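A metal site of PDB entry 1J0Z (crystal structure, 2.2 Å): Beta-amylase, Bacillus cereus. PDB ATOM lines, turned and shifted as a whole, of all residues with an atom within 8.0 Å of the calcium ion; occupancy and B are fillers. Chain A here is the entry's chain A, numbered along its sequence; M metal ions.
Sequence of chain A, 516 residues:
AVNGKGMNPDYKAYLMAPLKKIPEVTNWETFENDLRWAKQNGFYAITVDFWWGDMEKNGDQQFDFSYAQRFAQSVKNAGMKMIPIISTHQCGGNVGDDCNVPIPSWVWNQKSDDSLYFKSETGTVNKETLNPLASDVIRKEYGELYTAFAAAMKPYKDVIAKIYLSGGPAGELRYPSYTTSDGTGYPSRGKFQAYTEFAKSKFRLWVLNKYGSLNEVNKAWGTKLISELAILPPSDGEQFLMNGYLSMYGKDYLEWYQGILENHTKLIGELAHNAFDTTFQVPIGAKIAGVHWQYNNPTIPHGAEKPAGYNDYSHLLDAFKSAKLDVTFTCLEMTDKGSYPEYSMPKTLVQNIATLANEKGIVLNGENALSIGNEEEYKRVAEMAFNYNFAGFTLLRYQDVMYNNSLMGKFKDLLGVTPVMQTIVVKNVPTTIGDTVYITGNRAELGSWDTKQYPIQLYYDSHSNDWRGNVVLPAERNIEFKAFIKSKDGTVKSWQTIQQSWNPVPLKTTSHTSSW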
ATOM      1  N   TRP A  52      10.291 -18.364   2.924  1.00  0.00           N
ATOM      2  CA  TRP A  52       8.860 -18.519   3.135  1.00  0.00           C
ATOM      3  C   TRP A  52       8.131 -17.691   2.078  1.00  0.00           C
ATOM      4  O   TRP A  52       7.105 -18.118   1.528  1.00  0.00           O
ATOM      5  CB  TRP A  52       8.479 -18.056   4.550  1.00  0.00           C
ATOM      6  CG  TRP A  52       7.060 -18.378   4.934  1.00  0.00           C
ATOM      7  CD1 TRP A  52       6.192 -19.184   4.259  1.00  0.00           C
ATOM      8  CD2 TRP A  52       6.323 -17.865   6.060  1.00  0.00           C
ATOM      9  NE1 TRP A  52       4.971 -19.193   4.874  1.00  0.00           N
ATOM     10  CE2 TRP A  52       5.025 -18.397   5.984  1.00  0.00           C
ATOM     11  CE3 TRP A  52       6.642 -17.010   7.125  1.00  0.00           C
ATOM     12  CZ2 TRP A  52       4.029 -18.094   6.925  1.00  0.00           C
ATOM     13  CZ3 TRP A  52       5.656 -16.709   8.063  1.00  0.00           C
ATOM     14  CH2 TRP A  52       4.366 -17.252   7.948  1.00  0.00           C
ATOM     15  N   GLU A  56       5.243 -20.080  -0.066  1.00  0.00           N
ATOM     16  CA  GLU A  56       3.821 -19.923   0.194  1.00  0.00           C
ATOM     17  C   GLU A  56       3.439 -18.488  -0.108  1.00  0.00           C
ATOM     18  O   GLU A  56       2.696 -17.837   0.623  1.00  0.00           O
ATOM     19  CB  GLU A  56       3.513 -20.290   1.654  1.00  0.00           C
ATOM     20  CG  GLU A  56       2.067 -20.671   1.913  1.00  0.00           C
ATOM     21  CD  GLU A  56       1.790 -21.000   3.379  1.00  0.00           C
ATOM     22  OE1 GLU A  56       2.756 -21.148   4.172  1.00  0.00           O
ATOM     23  OE2 GLU A  56       0.603 -21.111   3.742  1.00  0.00           O
ATOM     24  N   GLY A  59      -0.800 -17.437  -1.354  1.00  0.00           N
ATOM     25  CA  GLY A  59      -1.858 -17.524  -0.366  1.00  0.00           C
ATOM     26  C   GLY A  59      -1.685 -18.693   0.569  1.00  0.00           C
ATOM     27  O   GLY A  59      -0.791 -19.509   0.390  1.00  0.00           O
ATOM     28  N   ASP A  60      -2.564 -18.751   1.572  1.00  0.00           N
ATOM     29  CA  ASP A  60      -2.524 -19.810   2.551  1.00  0.00           C
ATOM     30  C   ASP A  60      -2.665 -21.178   1.884  1.00  0.00           C
ATOM     31  O   ASP A  60      -3.621 -21.428   1.139  1.00  0.00           O
ATOM     32  CB  ASP A  60      -3.640 -19.593   3.585  1.00  0.00           C
ATOM     33  CG  ASP A  60      -3.561 -20.569   4.751  1.00  0.00           C
ATOM     34  OD1 ASP A  60      -2.460 -21.062   5.051  1.00  0.00           O
ATOM     35  OD2 ASP A  60      -4.599 -20.825   5.381  1.00  0.00           O
ATOM     36  N   GLN A  61      -1.698 -22.035   2.147  1.00  0.00           N
ATOM     37  CA  GLN A  61      -1.640 -23.393   1.615  1.00  0.00           C
ATOM     38  C   GLN A  61      -1.399 -23.457   0.108  1.00  0.00           C
ATOM     39  O   GLN A  61      -1.637 -24.492  -0.524  1.00  0.00           O
ATOM     40  CB  GLN A  61      -2.871 -24.200   2.034  1.00  0.00           C
ATOM     41  CG  GLN A  61      -3.096 -24.277   3.559  1.00  0.00           C
ATOM     42  CD  GLN A  61      -1.911 -24.869   4.312  1.00  0.00           C
ATOM     43  OE1 GLN A  61      -0.942 -24.178   4.606  1.00  0.00           O
ATOM     44  NE2 GLN A  61      -1.985 -26.153   4.610  1.00  0.00           N
ATOM     45  N   GLN A  62      -0.932 -22.356  -0.463  1.00  0.00           N
ATOM     46  CA  GLN A  62      -0.612 -22.322  -1.882  1.00  0.00           C
ATOM     47  C   GLN A  62       0.915 -22.418  -1.967  1.00  0.00           C
ATOM     48  O   GLN A  62       1.617 -21.433  -2.177  1.00  0.00           O
ATOM     49  CB  GLN A  62      -1.137 -21.043  -2.534  1.00  0.00           C
ATOM     50  CG  GLN A  62      -2.652 -20.953  -2.512  1.00  0.00           C
ATOM     51  CD  GLN A  62      -3.185 -19.734  -3.220  1.00  0.00           C
ATOM     52  OE1 GLN A  62      -2.703 -19.366  -4.288  1.00  0.00           O
ATOM     53  NE2 GLN A  62      -4.182 -19.096  -2.623  1.00  0.00           N
ATOM     54  N   PHE A  63       1.402 -23.642  -1.760  1.00  0.00           N
ATOM     55  CA  PHE A  63       2.834 -23.959  -1.744  1.00  0.00           C
ATOM     56  C   PHE A  63       3.522 -24.120  -3.098  1.00  0.00           C
ATOM     57  O   PHE A  63       2.923 -24.566  -4.083  1.00  0.00           O
ATOM     58  CB  PHE A  63       3.076 -25.229  -0.939  1.00  0.00           C
ATOM     59  CG  PHE A  63       2.573 -25.167   0.473  1.00  0.00           C
ATOM     60  CD1 PHE A  63       1.546 -26.009   0.885  1.00  0.00           C
ATOM     61  CD2 PHE A  63       3.142 -24.300   1.394  1.00  0.00           C
ATOM     62  CE1 PHE A  63       1.093 -25.985   2.203  1.00  0.00           C
ATOM     63  CE2 PHE A  63       2.702 -24.264   2.707  1.00  0.00           C
ATOM     64  CZ  PHE A  63       1.671 -25.113   3.114  1.00  0.00           C
ATOM     65  N   TRP A 106      -0.037 -11.912   2.574  1.00  0.00           N
ATOM     66  CA  TRP A 106      -1.371 -12.303   3.051  1.00  0.00           C
ATOM     67  C   TRP A 106      -1.394 -12.655   4.534  1.00  0.00           C
ATOM     68  O   TRP A 106      -2.465 -12.703   5.143  1.00  0.00           O
ATOM     69  CB  TRP A 106      -1.933 -13.479   2.209  1.00  0.00           C
ATOM     70  CG  TRP A 106      -1.054 -14.694   2.217  1.00  0.00           C
ATOM     71  CD1 TRP A 106      -0.085 -15.011   1.306  1.00  0.00           C
ATOM     72  CD2 TRP A 106      -1.001 -15.696   3.237  1.00  0.00           C
ATOM     73  NE1 TRP A 106       0.580 -16.146   1.698  1.00  0.00           N
ATOM     74  CE2 TRP A 106       0.042 -16.589   2.891  1.00  0.00           C
ATOM     75  CE3 TRP A 106      -1.718 -15.928   4.422  1.00  0.00           C
ATOM     76  CZ2 TRP A 106       0.377 -17.698   3.677  1.00  0.00           C
ATOM     77  CZ3 TRP A 106      -1.379 -17.024   5.207  1.00  0.00           C
ATOM     78  CH2 TRP A 106      -0.339 -17.889   4.833  1.00  0.00           C
ATOM     79  N   VAL A 107      -0.227 -12.914   5.109  1.00  0.00           N
ATOM     80  CA  VAL A 107      -0.151 -13.269   6.527  1.00  0.00           C
ATOM     81  C   VAL A 107      -0.517 -12.086   7.424  1.00  0.00           C
ATOM     82  O   VAL A 107      -1.157 -12.257   8.456  1.00  0.00           O
ATOM     83  CB  VAL A 107       1.250 -13.818   6.918  1.00  0.00           C
ATOM     84  CG1 VAL A 107       2.267 -12.693   7.001  1.00  0.00           C
ATOM     85  CG2 VAL A 107       1.161 -14.556   8.242  1.00  0.00           C
ATOM     86  N   GLN A 110      -4.155 -11.684   8.528  1.00  0.00           N
ATOM     87  CA  GLN A 110      -4.717 -12.642   9.478  1.00  0.00           C
ATOM     88  C   GLN A 110      -5.205 -11.984  10.769  1.00  0.00           C
ATOM     89  O   GLN A 110      -6.144 -12.456  11.393  1.00  0.00           O
ATOM     90  CB  GLN A 110      -3.697 -13.738   9.815  1.00  0.00           C
ATOM     91  CG  GLN A 110      -3.145 -14.506   8.608  1.00  0.00           C
ATOM     92  CD  GLN A 110      -4.224 -15.203   7.816  1.00  0.00           C
ATOM     93  OE1 GLN A 110      -4.633 -16.315   8.150  1.00  0.00           O
ATOM     94  NE2 GLN A 110      -4.682 -14.563   6.741  1.00  0.00           N
ATOM     95  N   VAL A 137      -0.763 -17.964  15.581  1.00  0.00           N
ATOM     96  CA  VAL A 137      -0.505 -17.860  14.149  1.00  0.00           C
ATOM     97  C   VAL A 137       0.779 -18.623  13.802  1.00  0.00           C
ATOM     98  O   VAL A 137       0.850 -19.296  12.775  1.00  0.00           O
ATOM     99  CB  VAL A 137      -0.343 -16.386  13.709  1.00  0.00           C
ATOM    100  CG1 VAL A 137       0.036 -16.295  12.229  1.00  0.00           C
ATOM    101  CG2 VAL A 137      -1.632 -15.621  13.962  1.00  0.00           C
ATOM    102  N   LYS A 140       0.003 -22.350  13.729  1.00  0.00           N
ATOM    103  CA  LYS A 140      -0.716 -22.725  12.528  1.00  0.00           C
ATOM    104  C   LYS A 140       0.186 -22.693  11.290  1.00  0.00           C
ATOM    105  O   LYS A 140       0.344 -23.704  10.613  1.00  0.00           O
ATOM    106  CB  LYS A 140      -1.901 -21.792  12.297  1.00  0.00           C
ATOM    107  CG  LYS A 140      -2.573 -22.019  10.958  1.00  0.00           C
ATOM    108  CD  LYS A 140      -3.713 -21.046  10.706  1.00  0.00           C
ATOM    109  CE  LYS A 140      -4.362 -21.299   9.353  1.00  0.00           C
ATOM    110  NZ  LYS A 140      -3.435 -21.065   8.197  1.00  0.00           N
ATOM    111  N   GLU A 141       0.807 -21.548  11.044  1.00  0.00           N
ATOM    112  CA  GLU A 141       1.653 -21.377   9.873  1.00  0.00           C
ATOM    113  C   GLU A 141       2.942 -22.189   9.811  1.00  0.00           C
ATOM    114  O   GLU A 141       3.254 -22.761   8.768  1.00  0.00           O
ATOM    115  CB  GLU A 141       1.951 -19.889   9.644  1.00  0.00           C
ATOM    116  CG  GLU A 141       0.697 -19.029   9.528  1.00  0.00           C
ATOM    117  CD  GLU A 141      -0.245 -19.462   8.411  1.00  0.00           C
ATOM    118  OE1 GLU A 141       0.197 -20.143   7.463  1.00  0.00           O
ATOM    119  OE2 GLU A 141      -1.438 -19.098   8.453  1.00  0.00           O
ATOM    120  N   TYR A 142       3.705 -22.241  10.904  1.00  0.00           N
ATOM    121  CA  TYR A 142       4.943 -23.002  10.922  1.00  0.00           C
ATOM    122  C   TYR A 142       4.649 -24.490  10.901  1.00  0.00           C
ATOM    123  O   TYR A 142       5.366 -25.266  10.287  1.00  0.00           O
ATOM    124  CB  TYR A 142       5.821 -22.637  12.130  1.00  0.00           C
ATOM    125  CG  TYR A 142       6.443 -21.250  12.075  1.00  0.00           C
ATOM    126  CD1 TYR A 142       5.820 -20.198  11.406  1.00  0.00           C
ATOM    127  CD2 TYR A 142       7.649 -20.984  12.750  1.00  0.00           C
ATOM    128  CE1 TYR A 142       6.368 -18.923  11.401  1.00  0.00           C
ATOM    129  CE2 TYR A 142       8.197 -19.709  12.744  1.00  0.00           C
ATOM    130  CZ  TYR A 142       7.549 -18.673  12.075  1.00  0.00           C
ATOM    131  OH  TYR A 142       8.069 -17.405  12.092  1.00  0.00           O
ATOM    132  N   GLY A 143       3.602 -24.891  11.613  1.00  0.00           N
ATOM    133  CA  GLY A 143       3.218 -26.287  11.616  1.00  0.00           C
ATOM    134  C   GLY A 143       2.888 -26.690  10.196  1.00  0.00           C
ATOM    135  O   GLY A 143       3.439 -27.658   9.672  1.00  0.00           O
ATOM    136  N   GLU A 144       2.042 -25.887   9.538  1.00  0.00           N
ATOM    137  CA  GLU A 144       1.613 -26.130   8.167  1.00  0.00           C
ATOM    138  C   GLU A 144       2.778 -26.137   7.179  1.00  0.00           C
ATOM    139  O   GLU A 144       2.873 -27.050   6.350  1.00  0.00           O
ATOM    140  CB  GLU A 144       0.575 -25.108   7.748  1.00  0.00           C
ATOM    141  CG  GLU A 144      -0.783 -25.304   8.401  1.00  0.00           C
ATOM    142  CD  GLU A 144      -1.810 -24.238   8.023  1.00  0.00           C
ATOM    143  OE1 GLU A 144      -1.416 -23.110   7.664  1.00  0.00           O
ATOM    144  OE2 GLU A 144      -3.020 -24.526   8.105  1.00  0.00           O
ATOM    145  N   LEU A 145       3.663 -25.164   7.291  1.00  0.00           N
ATOM    146  CA  LEU A 145       4.831 -25.051   6.405  1.00  0.00           C
ATOM    147  C   LEU A 145       5.859 -26.168   6.636  1.00  0.00           C
ATOM    148  O   LEU A 145       6.399 -26.725   5.675  1.00  0.00           O
ATOM    149  CB  LEU A 145       5.490 -23.681   6.566  1.00  0.00           C
ATOM    150  CG  LEU A 145       6.704 -23.367   5.689  1.00  0.00           C
ATOM    151  CD1 LEU A 145       6.297 -23.337   4.217  1.00  0.00           C
ATOM    152  CD2 LEU A 145       7.300 -22.034   6.111  1.00  0.00           C
ATOM    153  N   ALA A 148       4.369 -29.401   5.295  1.00  0.00           N
ATOM    154  CA  ALA A 148       4.316 -29.364   3.834  1.00  0.00           C
ATOM    155  C   ALA A 148       5.720 -29.572   3.248  1.00  0.00           C
ATOM    156  O   ALA A 148       5.892 -30.375   2.340  1.00  0.00           O
ATOM    157  CB  ALA A 148       3.732 -28.049   3.361  1.00  0.00           C
HETATM  158 CA    CA M   1      -0.404 -21.920   5.824  1.00  0.00          CA
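The side-chain carboxylate of Asp 60 is in salt-bridge range of the side-chain amino group of Lys 140, 3.1 Å away.
The side-chain carboxylate of Glu 144 is in salt-bridge range of the side-chain amino group of Lys 140, 3.5 Å away.
NE1 of Trp 106 is in hydrogen-bond range of O of Glu 56 (2.9 Å).
The indole nitrogen (NE1) of Trp 52 is in hydrogen-bond range of the side-chain carboxylate (OE1) of Glu 56.
The side-chain carboxylate (OE2) of Glu 141 is in salt-bridge range of the side-chain amino group (NZ) of Lys 140.
Merely in contact with the calcium ion: Lys 140 (3.9 Å).
The nearest printed residue that does not touch the calcium ion is Trp 106 (4.2 Å).
The calcium ion is bound by OD1 of Asp 60 (2.4 Å), OE1 of Glu 144 (2.4 Å), OE2 of Glu 56 (2.5 Å), OE1 of Glu 141 (2.5 Å) and OE1 of Gln 61 (2.6 Å).
The calcium ion has five donor atoms within binding distance.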
